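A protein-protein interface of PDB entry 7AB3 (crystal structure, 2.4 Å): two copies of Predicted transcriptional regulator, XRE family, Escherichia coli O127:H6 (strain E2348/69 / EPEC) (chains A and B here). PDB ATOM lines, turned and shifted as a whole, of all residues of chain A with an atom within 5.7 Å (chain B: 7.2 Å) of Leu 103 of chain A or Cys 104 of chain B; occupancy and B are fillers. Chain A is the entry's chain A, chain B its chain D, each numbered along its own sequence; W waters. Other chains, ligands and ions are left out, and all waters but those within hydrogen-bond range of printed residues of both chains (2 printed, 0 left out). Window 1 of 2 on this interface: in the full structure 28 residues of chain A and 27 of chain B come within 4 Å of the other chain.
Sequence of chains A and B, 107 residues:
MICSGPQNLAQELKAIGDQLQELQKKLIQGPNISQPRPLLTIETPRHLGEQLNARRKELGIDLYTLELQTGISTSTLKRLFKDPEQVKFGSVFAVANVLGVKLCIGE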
ATOM      1  N   LEU A  39       4.409 -19.015  24.608  1.00  0.00           N
ATOM      2  CA  LEU A  39       4.734 -19.670  23.337  1.00  0.00           C
ATOM      3  C   LEU A  39       6.064 -20.420  23.379  1.00  0.00           C
ATOM      4  O   LEU A  39       7.101 -19.819  23.657  1.00  0.00           O
ATOM      5  CB  LEU A  39       4.796 -18.595  22.258  1.00  0.00           C
ATOM      6  CG  LEU A  39       4.364 -18.937  20.850  1.00  0.00           C
ATOM      7  CD1 LEU A  39       3.089 -19.786  20.820  1.00  0.00           C
ATOM      8  CD2 LEU A  39       4.184 -17.667  20.047  1.00  0.00           C
ATOM      9  N   LEU A  40       6.046 -21.730  23.116  1.00  0.00           N
ATOM     10  CA  LEU A  40       7.250 -22.541  23.160  1.00  0.00           C
ATOM     11  C   LEU A  40       7.552 -23.154  21.801  1.00  0.00           C
ATOM     12  O   LEU A  40       6.719 -23.881  21.259  1.00  0.00           O
ATOM     13  CB  LEU A  40       7.050 -23.663  24.193  1.00  0.00           C
ATOM     14  CG  LEU A  40       8.178 -24.675  24.329  1.00  0.00           C
ATOM     15  CD1 LEU A  40       9.409 -24.040  24.953  1.00  0.00           C
ATOM     16  CD2 LEU A  40       7.723 -25.867  25.127  1.00  0.00           C
ATOM     17  N   THR A  41       8.745 -22.881  21.251  1.00  0.00           N
ATOM     18  CA  THR A  41       9.148 -23.477  19.981  1.00  0.00           C
ATOM     19  C   THR A  41       9.510 -24.933  20.251  1.00  0.00           C
ATOM     20  O   THR A  41      10.287 -25.199  21.169  1.00  0.00           O
ATOM     21  CB  THR A  41      10.304 -22.682  19.347  1.00  0.00           C
ATOM     22  OG1 THR A  41       9.831 -21.369  19.070  1.00  0.00           O
ATOM     23  CG2 THR A  41      10.811 -23.295  18.052  1.00  0.00           C
ATOM     24  N   ILE A  42       8.938 -25.874  19.492  1.00  0.00           N
ATOM     25  CA  ILE A  42       9.235 -27.275  19.739  1.00  0.00           C
ATOM     26  C   ILE A  42      10.509 -27.603  18.942  1.00  0.00           C
ATOM     27  O   ILE A  42      10.582 -27.352  17.731  1.00  0.00           O
ATOM     28  CB  ILE A  42       8.014 -28.253  19.599  1.00  0.00           C
ATOM     29  CG1 ILE A  42       7.971 -28.946  18.276  1.00  0.00           C
ATOM     30  CG2 ILE A  42       6.672 -27.595  19.910  1.00  0.00           C
ATOM     31  CD1 ILE A  42       8.410 -30.263  18.448  1.00  0.00           C
ATOM     32  N   LEU A  48       8.141 -32.176  22.045  1.00  0.00           N
ATOM     33  CA  LEU A  48       6.697 -32.089  22.027  1.00  0.00           C
ATOM     34  C   LEU A  48       6.035 -33.190  22.864  1.00  0.00           C
ATOM     35  O   LEU A  48       5.140 -32.889  23.647  1.00  0.00           O
ATOM     36  CB  LEU A  48       6.157 -32.090  20.604  1.00  0.00           C
ATOM     37  CG  LEU A  48       4.639 -31.950  20.517  1.00  0.00           C
ATOM     38  CD1 LEU A  48       4.168 -30.634  21.099  1.00  0.00           C
ATOM     39  CD2 LEU A  48       4.169 -32.161  19.147  1.00  0.00           C
ATOM     40  N   PHE A  89       0.865 -38.081  12.619  1.00  0.00           N
ATOM     41  CA  PHE A  89       0.658 -36.671  12.937  1.00  0.00           C
ATOM     42  C   PHE A  89      -0.734 -36.415  13.517  1.00  0.00           C
ATOM     43  O   PHE A  89      -0.851 -35.674  14.496  1.00  0.00           O
ATOM     44  CB  PHE A  89       0.956 -35.756  11.727  1.00  0.00           C
ATOM     45  CG  PHE A  89       0.691 -34.296  12.028  1.00  0.00           C
ATOM     46  CD1 PHE A  89       1.594 -33.550  12.750  1.00  0.00           C
ATOM     47  CD2 PHE A  89      -0.510 -33.705  11.677  1.00  0.00           C
ATOM     48  CE1 PHE A  89       1.323 -32.229  13.082  1.00  0.00           C
ATOM     49  CE2 PHE A  89      -0.791 -32.394  12.044  1.00  0.00           C
ATOM     50  CZ  PHE A  89       0.133 -31.665  12.735  1.00  0.00           C
ATOM     51  N   PHE A  93      -1.754 -34.544  16.956  1.00  0.00           N
ATOM     52  CA  PHE A  93      -2.661 -33.411  16.871  1.00  0.00           C
ATOM     53  C   PHE A  93      -3.968 -33.626  17.711  1.00  0.00           C
ATOM     54  O   PHE A  93      -4.433 -32.697  18.373  1.00  0.00           O
ATOM     55  CB  PHE A  93      -2.955 -33.094  15.398  1.00  0.00           C
ATOM     56  CG  PHE A  93      -3.666 -31.782  15.183  1.00  0.00           C
ATOM     57  CD1 PHE A  93      -2.958 -30.596  15.116  1.00  0.00           C
ATOM     58  CD2 PHE A  93      -5.051 -31.731  15.077  1.00  0.00           C
ATOM     59  CE1 PHE A  93      -3.615 -29.381  14.952  1.00  0.00           C
ATOM     60  CE2 PHE A  93      -5.708 -30.516  14.929  1.00  0.00           C
ATOM     61  CZ  PHE A  93      -4.982 -29.352  14.856  1.00  0.00           C
ATOM     62  N   ALA A  96      -2.910 -33.303  21.486  1.00  0.00           N
ATOM     63  CA  ALA A  96      -2.676 -31.892  21.811  1.00  0.00           C
ATOM     64  C   ALA A  96      -4.018 -31.155  21.990  1.00  0.00           C
ATOM     65  O   ALA A  96      -4.157 -30.311  22.854  1.00  0.00           O
ATOM     66  CB  ALA A  96      -1.864 -31.238  20.708  1.00  0.00           C
ATOM     67  N   VAL A 101      -3.978 -27.794  24.200  1.00  0.00           N
ATOM     68  CA  VAL A 101      -2.740 -27.260  23.658  1.00  0.00           C
ATOM     69  C   VAL A 101      -2.940 -26.890  22.194  1.00  0.00           C
ATOM     70  O   VAL A 101      -3.415 -27.701  21.395  1.00  0.00           O
ATOM     71  CB  VAL A 101      -1.605 -28.312  23.822  1.00  0.00           C
ATOM     72  CG1 VAL A 101      -0.291 -27.831  23.199  1.00  0.00           C
ATOM     73  CG2 VAL A 101      -1.417 -28.688  25.283  1.00  0.00           C
ATOM     74  N   LYS A 102      -2.590 -25.655  21.834  1.00  0.00           N
ATOM     75  CA  LYS A 102      -2.692 -25.195  20.458  1.00  0.00           C
ATOM     76  C   LYS A 102      -1.345 -25.338  19.740  1.00  0.00           C
ATOM     77  O   LYS A 102      -0.301 -25.082  20.322  1.00  0.00           O
ATOM     78  CB  LYS A 102      -3.164 -23.736  20.411  1.00  0.00           C
ATOM     79  CG  LYS A 102      -4.648 -23.568  20.624  1.00  0.00           C
ATOM     80  CD  LYS A 102      -5.008 -22.093  20.629  1.00  0.00           C
ATOM     81  CE  LYS A 102      -6.495 -21.892  20.792  1.00  0.00           C
ATOM     82  NZ  LYS A 102      -6.798 -20.531  21.303  1.00  0.00           N
ATOM     83  N   LEU A 103      -1.392 -25.754  18.477  1.00  0.00           N
ATOM     84  CA  LEU A 103      -0.239 -25.905  17.602  1.00  0.00           C
ATOM     85  C   LEU A 103      -0.186 -24.659  16.724  1.00  0.00           C
ATOM     86  O   LEU A 103      -1.187 -24.289  16.136  1.00  0.00           O
ATOM     87  CB  LEU A 103      -0.440 -27.108  16.697  1.00  0.00           C
ATOM     88  CG  LEU A 103       0.750 -28.014  16.541  1.00  0.00           C
ATOM     89  CD1 LEU A 103       0.767 -29.077  17.658  1.00  0.00           C
ATOM     90  CD2 LEU A 103       0.745 -28.648  15.140  1.00  0.00           C
ATOM     91  N   CYS A 104       0.967 -24.003  16.649  1.00  0.00           N
ATOM     92  CA  CYS A 104       1.137 -22.804  15.845  1.00  0.00           C
ATOM     93  C   CYS A 104       2.312 -22.991  14.877  1.00  0.00           C
ATOM     94  O   CYS A 104       3.169 -23.845  15.093  1.00  0.00           O
ATOM     95  CB  CYS A 104       1.364 -21.582  16.738  1.00  0.00           C
ATOM     96  SG  CYS A 104       0.173 -21.387  18.093  1.00  0.00           S
ATOM     97  N   ILE A 105       2.354 -22.179  13.815  1.00  0.00           N
ATOM     98  CA  ILE A 105       3.483 -22.158  12.888  1.00  0.00           C
ATOM     99  C   ILE A 105       4.009 -20.731  12.731  1.00  0.00           C
ATOM    100  O   ILE A 105       3.250 -19.772  12.722  1.00  0.00           O
ATOM    101  CB  ILE A 105       3.294 -22.877  11.522  1.00  0.00           C
ATOM    102  CG1 ILE A 105       2.094 -22.383  10.763  1.00  0.00           C
ATOM    103  CG2 ILE A 105       3.266 -24.384  11.682  1.00  0.00           C
ATOM    104  CD1 ILE A 105       2.141 -22.763   9.309  1.00  0.00           C
ATOM    105  N   GLY A 106       5.322 -20.619  12.672  1.00  0.00           N
ATOM    106  CA  GLY A 106       6.030 -19.357  12.483  1.00  0.00           C
ATOM    107  C   GLY A 106       7.266 -19.543  11.626  1.00  0.00           C
ATOM    108  O   GLY A 106       7.417 -20.578  10.979  1.00  0.00           O
ATOM    109  N   LEU B  39       2.520 -15.596  13.697  1.00  0.00           N
ATOM    110  CA  LEU B  39       2.097 -16.912  14.194  1.00  0.00           C
ATOM    111  C   LEU B  39       0.707 -17.321  13.654  1.00  0.00           C
ATOM    112  O   LEU B  39      -0.248 -16.550  13.720  1.00  0.00           O
ATOM    113  CB  LEU B  39       2.174 -17.027  15.751  1.00  0.00           C
ATOM    114  CG  LEU B  39       1.071 -16.331  16.590  1.00  0.00           C
ATOM    115  CD1 LEU B  39       0.036 -17.331  17.118  1.00  0.00           C
ATOM    116  CD2 LEU B  39       1.679 -15.531  17.765  1.00  0.00           C
ATOM    117  N   LEU B  40       0.599 -18.542  13.153  1.00  0.00           N
ATOM    118  CA  LEU B  40      -0.650 -19.060  12.608  1.00  0.00           C
ATOM    119  C   LEU B  40      -1.080 -20.307  13.373  1.00  0.00           C
ATOM    120  O   LEU B  40      -0.348 -21.300  13.385  1.00  0.00           O
ATOM    121  CB  LEU B  40      -0.457 -19.410  11.127  1.00  0.00           C
ATOM    122  CG  LEU B  40      -1.657 -20.059  10.431  1.00  0.00           C
ATOM    123  CD1 LEU B  40      -2.817 -19.078  10.288  1.00  0.00           C
ATOM    124  CD2 LEU B  40      -1.266 -20.617   9.097  1.00  0.00           C
ATOM    125  N   THR B  41      -2.272 -20.270  13.987  1.00  0.00           N
ATOM    126  CA  THR B  41      -2.788 -21.428  14.684  1.00  0.00           C
ATOM    127  C   THR B  41      -3.244 -22.454  13.661  1.00  0.00           C
ATOM    128  O   THR B  41      -4.002 -22.127  12.749  1.00  0.00           O
ATOM    129  CB  THR B  41      -3.913 -21.044  15.657  1.00  0.00           C
ATOM    130  OG1 THR B  41      -3.451 -20.024  16.554  1.00  0.00           O
ATOM    131  CG2 THR B  41      -4.430 -22.245  16.451  1.00  0.00           C
ATOM    132  N   ILE B  42      -2.744 -23.691  13.805  1.00  0.00           N
ATOM    133  CA  ILE B  42      -3.090 -24.851  12.984  1.00  0.00           C
ATOM    134  C   ILE B  42      -4.442 -25.372  13.410  1.00  0.00           C
ATOM    135  O   ILE B  42      -4.607 -25.846  14.539  1.00  0.00           O
ATOM    136  CB  ILE B  42      -2.002 -25.935  13.105  1.00  0.00           C
ATOM    137  CG1 ILE B  42      -0.639 -25.378  12.637  1.00  0.00           C
ATOM    138  CG2 ILE B  42      -2.401 -27.224  12.374  1.00  0.00           C
ATOM    139  CD1 ILE B  42      -0.675 -24.865  11.149  1.00  0.00           C
ATOM    140  N   GLU B  43      -5.417 -25.235  12.523  1.00  0.00           N
ATOM    141  CA  GLU B  43      -6.784 -25.648  12.761  1.00  0.00           C
ATOM    142  C   GLU B  43      -6.956 -27.191  12.673  1.00  0.00           C
ATOM    143  O   GLU B  43      -7.598 -27.781  13.548  1.00  0.00           O
ATOM    144  CB  GLU B  43      -7.739 -24.864  11.830  1.00  0.00           C
ATOM    145  CG  GLU B  43      -7.797 -23.379  12.175  1.00  0.00           C
ATOM    146  CD  GLU B  43      -8.513 -22.441  11.205  1.00  0.00           C
ATOM    147  OE1 GLU B  43      -9.503 -21.795  11.632  1.00  0.00           O
ATOM    148  OE2 GLU B  43      -8.080 -22.328  10.031  1.00  0.00           O
ATOM    149  N   THR B  44      -6.353 -27.839  11.653  1.00  0.00           N
ATOM    150  CA  THR B  44      -6.407 -29.293  11.427  1.00  0.00           C
ATOM    151  C   THR B  44      -5.103 -29.822  10.801  1.00  0.00           C
ATOM    152  O   THR B  44      -4.377 -29.026  10.224  1.00  0.00           O
ATOM    153  CB  THR B  44      -7.575 -29.669  10.450  1.00  0.00           C
ATOM    154  OG1 THR B  44      -7.322 -29.186   9.135  1.00  0.00           O
ATOM    155  CG2 THR B  44      -8.930 -29.223  10.911  1.00  0.00           C
ATOM    156  N   LEU B  48      -2.197 -27.631   8.110  1.00  0.00           N
ATOM    157  CA  LEU B  48      -0.752 -27.656   8.136  1.00  0.00           C
ATOM    158  C   LEU B  48      -0.129 -28.110   6.815  1.00  0.00           C
ATOM    159  O   LEU B  48       0.791 -27.456   6.337  1.00  0.00           O
ATOM    160  CB  LEU B  48      -0.227 -28.506   9.287  1.00  0.00           C
ATOM    161  CG  LEU B  48       1.290 -28.535   9.417  1.00  0.00           C
ATOM    162  CD1 LEU B  48       1.841 -27.147   9.681  1.00  0.00           C
ATOM    163  CD2 LEU B  48       1.716 -29.485  10.445  1.00  0.00           C
ATOM    164  N   PHE B  89       4.735 -38.186  12.417  1.00  0.00           N
ATOM    165  CA  PHE B  89       5.032 -36.854  12.962  1.00  0.00           C
ATOM    166  C   PHE B  89       6.434 -36.383  12.603  1.00  0.00           C
ATOM    167  O   PHE B  89       6.598 -35.237  12.222  1.00  0.00           O
ATOM    168  CB  PHE B  89       4.766 -36.778  14.495  1.00  0.00           C
ATOM    169  CG  PHE B  89       5.078 -35.406  15.057  1.00  0.00           C
ATOM    170  CD1 PHE B  89       4.189 -34.356  14.904  1.00  0.00           C
ATOM    171  CD2 PHE B  89       6.296 -35.140  15.641  1.00  0.00           C
ATOM    172  CE1 PHE B  89       4.515 -33.072  15.336  1.00  0.00           C
ATOM    173  CE2 PHE B  89       6.619 -33.852  16.058  1.00  0.00           C
ATOM    174  CZ  PHE B  89       5.721 -32.832  15.915  1.00  0.00           C
ATOM    175  N   LYS B 102       8.882 -22.911  11.811  1.00  0.00           N
ATOM    176  CA  LYS B 102       8.958 -23.300  13.207  1.00  0.00           C
ATOM    177  C   LYS B 102       7.579 -23.748  13.731  1.00  0.00           C
ATOM    178  O   LYS B 102       6.562 -23.133  13.429  1.00  0.00           O
ATOM    179  CB  LYS B 102       9.493 -22.155  14.068  1.00  0.00           C
ATOM    180  CG  LYS B 102      10.993 -22.043  14.011  1.00  0.00           C
ATOM    181  CD  LYS B 102      11.498 -20.898  14.880  1.00  0.00           C
ATOM    182  CE  LYS B 102      13.008 -20.774  14.843  1.00  0.00           C
ATOM    183  NZ  LYS B 102      13.462 -19.385  14.508  1.00  0.00           N
ATOM    184  N   LEU B 103       7.563 -24.822  14.506  1.00  0.00           N
ATOM    185  CA  LEU B 103       6.380 -25.370  15.149  1.00  0.00           C
ATOM    186  C   LEU B 103       6.381 -24.862  16.583  1.00  0.00           C
ATOM    187  O   LEU B 103       7.396 -24.963  17.266  1.00  0.00           O
ATOM    188  CB  LEU B 103       6.504 -26.883  15.197  1.00  0.00           C
ATOM    189  CG  LEU B 103       5.276 -27.664  14.838  1.00  0.00           C
ATOM    190  CD1 LEU B 103       5.251 -27.923  13.333  1.00  0.00           C
ATOM    191  CD2 LEU B 103       5.259 -28.979  15.605  1.00  0.00           C
ATOM    192  N   CYS B 104       5.266 -24.298  17.030  1.00  0.00           N
ATOM    193  CA  CYS B 104       5.152 -23.780  18.387  1.00  0.00           C
ATOM    194  C   CYS B 104       3.939 -24.381  19.091  1.00  0.00           C
ATOM    195  O   CYS B 104       3.038 -24.885  18.436  1.00  0.00           O
ATOM    196  CB  CYS B 104       5.078 -22.254  18.368  1.00  0.00           C
ATOM    197  SG  CYS B 104       6.510 -21.465  17.594  1.00  0.00           S
ATOM    198  N   ILE B 105       3.920 -24.320  20.428  1.00  0.00           N
ATOM    199  CA  ILE B 105       2.778 -24.744  21.217  1.00  0.00           C
ATOM    200  C   ILE B 105       2.359 -23.637  22.183  1.00  0.00           C
ATOM    201  O   ILE B 105       3.192 -22.948  22.754  1.00  0.00           O
ATOM    202  CB  ILE B 105       2.882 -26.130  21.913  1.00  0.00           C
ATOM    203  CG1 ILE B 105       4.112 -26.246  22.814  1.00  0.00           C
ATOM    204  CG2 ILE B 105       2.799 -27.275  20.909  1.00  0.00           C
ATOM    205  CD1 ILE B 105       4.074 -27.405  23.726  1.00  0.00           C
ATOM    206  N   GLY B 106       1.054 -23.472  22.319  1.00  0.00           N
ATOM    207  CA  GLY B 106       0.441 -22.489  23.201  1.00  0.00           C
ATOM    208  C   GLY B 106      -0.807 -23.042  23.870  1.00  0.00           C
ATOM    209  O   GLY B 106      -1.048 -24.252  23.838  1.00  0.00           O
ATOM    210  N   GLU B 107      -1.619 -22.171  24.495  1.00  0.00           N
ATOM    211  CA  GLU B 107      -2.845 -22.611  25.170  1.00  0.00           C
ATOM    212  C   GLU B 107      -4.051 -21.787  24.714  1.00  0.00           C
ATOM    213  O   GLU B 107      -4.946 -22.322  24.054  1.00  0.00           O
ATOM    214  CB  GLU B 107      -2.699 -22.594  26.718  1.00  0.00           C
ATOM    215  CG  GLU B 107      -2.444 -23.967  27.340  1.00  0.00           C
ATOM    216  CD  GLU B 107      -1.068 -24.209  27.948  1.00  0.00           C
ATOM    217  OE1 GLU B 107      -0.911 -23.937  29.161  1.00  0.00           O
ATOM    218  OE2 GLU B 107      -0.159 -24.690  27.229  1.00  0.00           O
HETATM  219  O   HOH W   1      10.006 -25.905  15.567  1.00  0.00           O
HETATM  220  O   HOH W   2      -4.023 -26.389  17.187  1.00  0.00           O
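Of the 14 printed residues of chain B, 14 touch a printed residue of chain A.
Hydrophobic or aromatic side chains of chain B that line the printed part of chain A: Leu 40, Ile 42, Leu 48, Phe 89, Leu 103 and Ile 105.
Among the printed residues, no Asp or Glu carboxylate lies within 4 Å of a Lys or Arg side-chain nitrogen of the other chain.
Printed residues of chain B within 4 Å of Leu 103 of chain A: Thr 41, Ile 42 and Cys 104.
Printed residues of chain A within 4 Å of Cys 104 of chain B: Leu 40 (3.3 Å), Thr 41 (3.6 Å), Lys 102 (3.8 Å), Leu 103 (3.5 Å) and Cys 104 (2.9 Å).
Of the printed residues of chain A, Glu 43 of chain B touches Phe 93.
Of the printed residues of chain A, Ile 42 of chain B touches Phe 93, Leu 103 and Ile 105.
Ala 96 of chain A touches none of the printed residues of chain B.
The nearest printed residue of chain A that does not touch Cys 104 of chain B is Leu 39 of chain A (4.01 Å).
The nearest printed residue of chain A that does not touch Ile 105 of chain B is Ile 42 of chain A (4.01 Å).
The backbone NH of Lys 102 of chain A is in hydrogen-bond range of the backbone carbonyl oxygen of Gly 106 of chain B.
N of Ile 105 of chain A sits at hydrogen-bond distance from O of Leu 40 of chain B, at 2.9 Å.
The backbone NH (N) of Ile 105 of chain B is in hydrogen-bond range of the backbone carbonyl oxygen (O) of Leu 40 of chain A (3.0 Å).
The backbone NH (N) of Cys 104 of chain A lies within hydrogen-bond range of the backbone carbonyl oxygen (O) of Cys 104 of chain B (2.9 Å).
OG1 of Thr 41 of chain A sits at hydrogen-bond distance from SG of Cys 104 of chain B, at 3.6 Å.
The backbone carbonyl oxygen of Gly 106 of chain A sits at hydrogen-bond distance from the backbone NH of Lys 102 of chain B, at 2.9 Å.
N of Ile 42 of chain A is in hydrogen-bond range of O of Leu 103 of chain B.
The backbone carbonyl oxygen of Leu 103 of chain A is in hydrogen-bond range of the backbone NH of Ile 42 of chain B (2.9 Å).
The backbone carbonyl oxygen (O) of Ala 96 of chain A lies within hydrogen-bond range of the backbone NH (N) of Val 101 of chain A, at 2.9 Å.
Thr 41 of chain A touches Cys 104 of chain B, but with the chains exchanged Cys 104 of chain A does not touch Thr 41 of chain B (4.2 Å).
Phe 89 of chain A touches its own counterpart, Phe 89 of chain B.
Lys 102 of chain A touches Gly 106 of chain B, and with the chains exchanged Gly 106 of chain A touches Lys 102 of chain B.
Ile 105 of chain A touches Ile 42 of chain B, but with the chains exchanged Ile 42 of chain A does not touch Ile 105 of chain B (4.01 Å).
Water W1 lies within hydrogen-bond range of O of Ile 42 of chain A (2.7 Å) and N of Leu 103 of chain B (2.9 Å).
Water W2 lies within hydrogen-bond range of the backbone carbonyl oxygen (O) of Ile 42 of chain B (2.8 Å) and the backbone NH (N) of Leu 103 of chain A (3.0 Å).
Cys 104 of chain B touches Leu 40 of chain A.
Leu 48 of chain A touches Phe 89 of chain B.
CZ of Phe 89 of chain A touches CD2 of Leu 48 of chain B, at 3.5 Å.
CZ of Phe 93 of chain A touches O of Glu 43 of chain B (3.3 Å).
Lys 102 of chain A touches Cys 104 of chain B (O to O, 3.8 Å).
O of Leu 103 of chain A touches CA of Thr 41 of chain B, at 3.6 Å.
CA of Leu 103 of chain A touches O of Cys 104 of chain B, 3.5 Å away.
Cys 104 of chain A touches Leu 40 of chain B (CA to O, 3.2 Å).
Leu 103 of chain B touches Cys 104 of chain A.
CG1 of Ile 105 of chain A touches CD1 of Ile 42 of chain B, 3.7 Å away.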
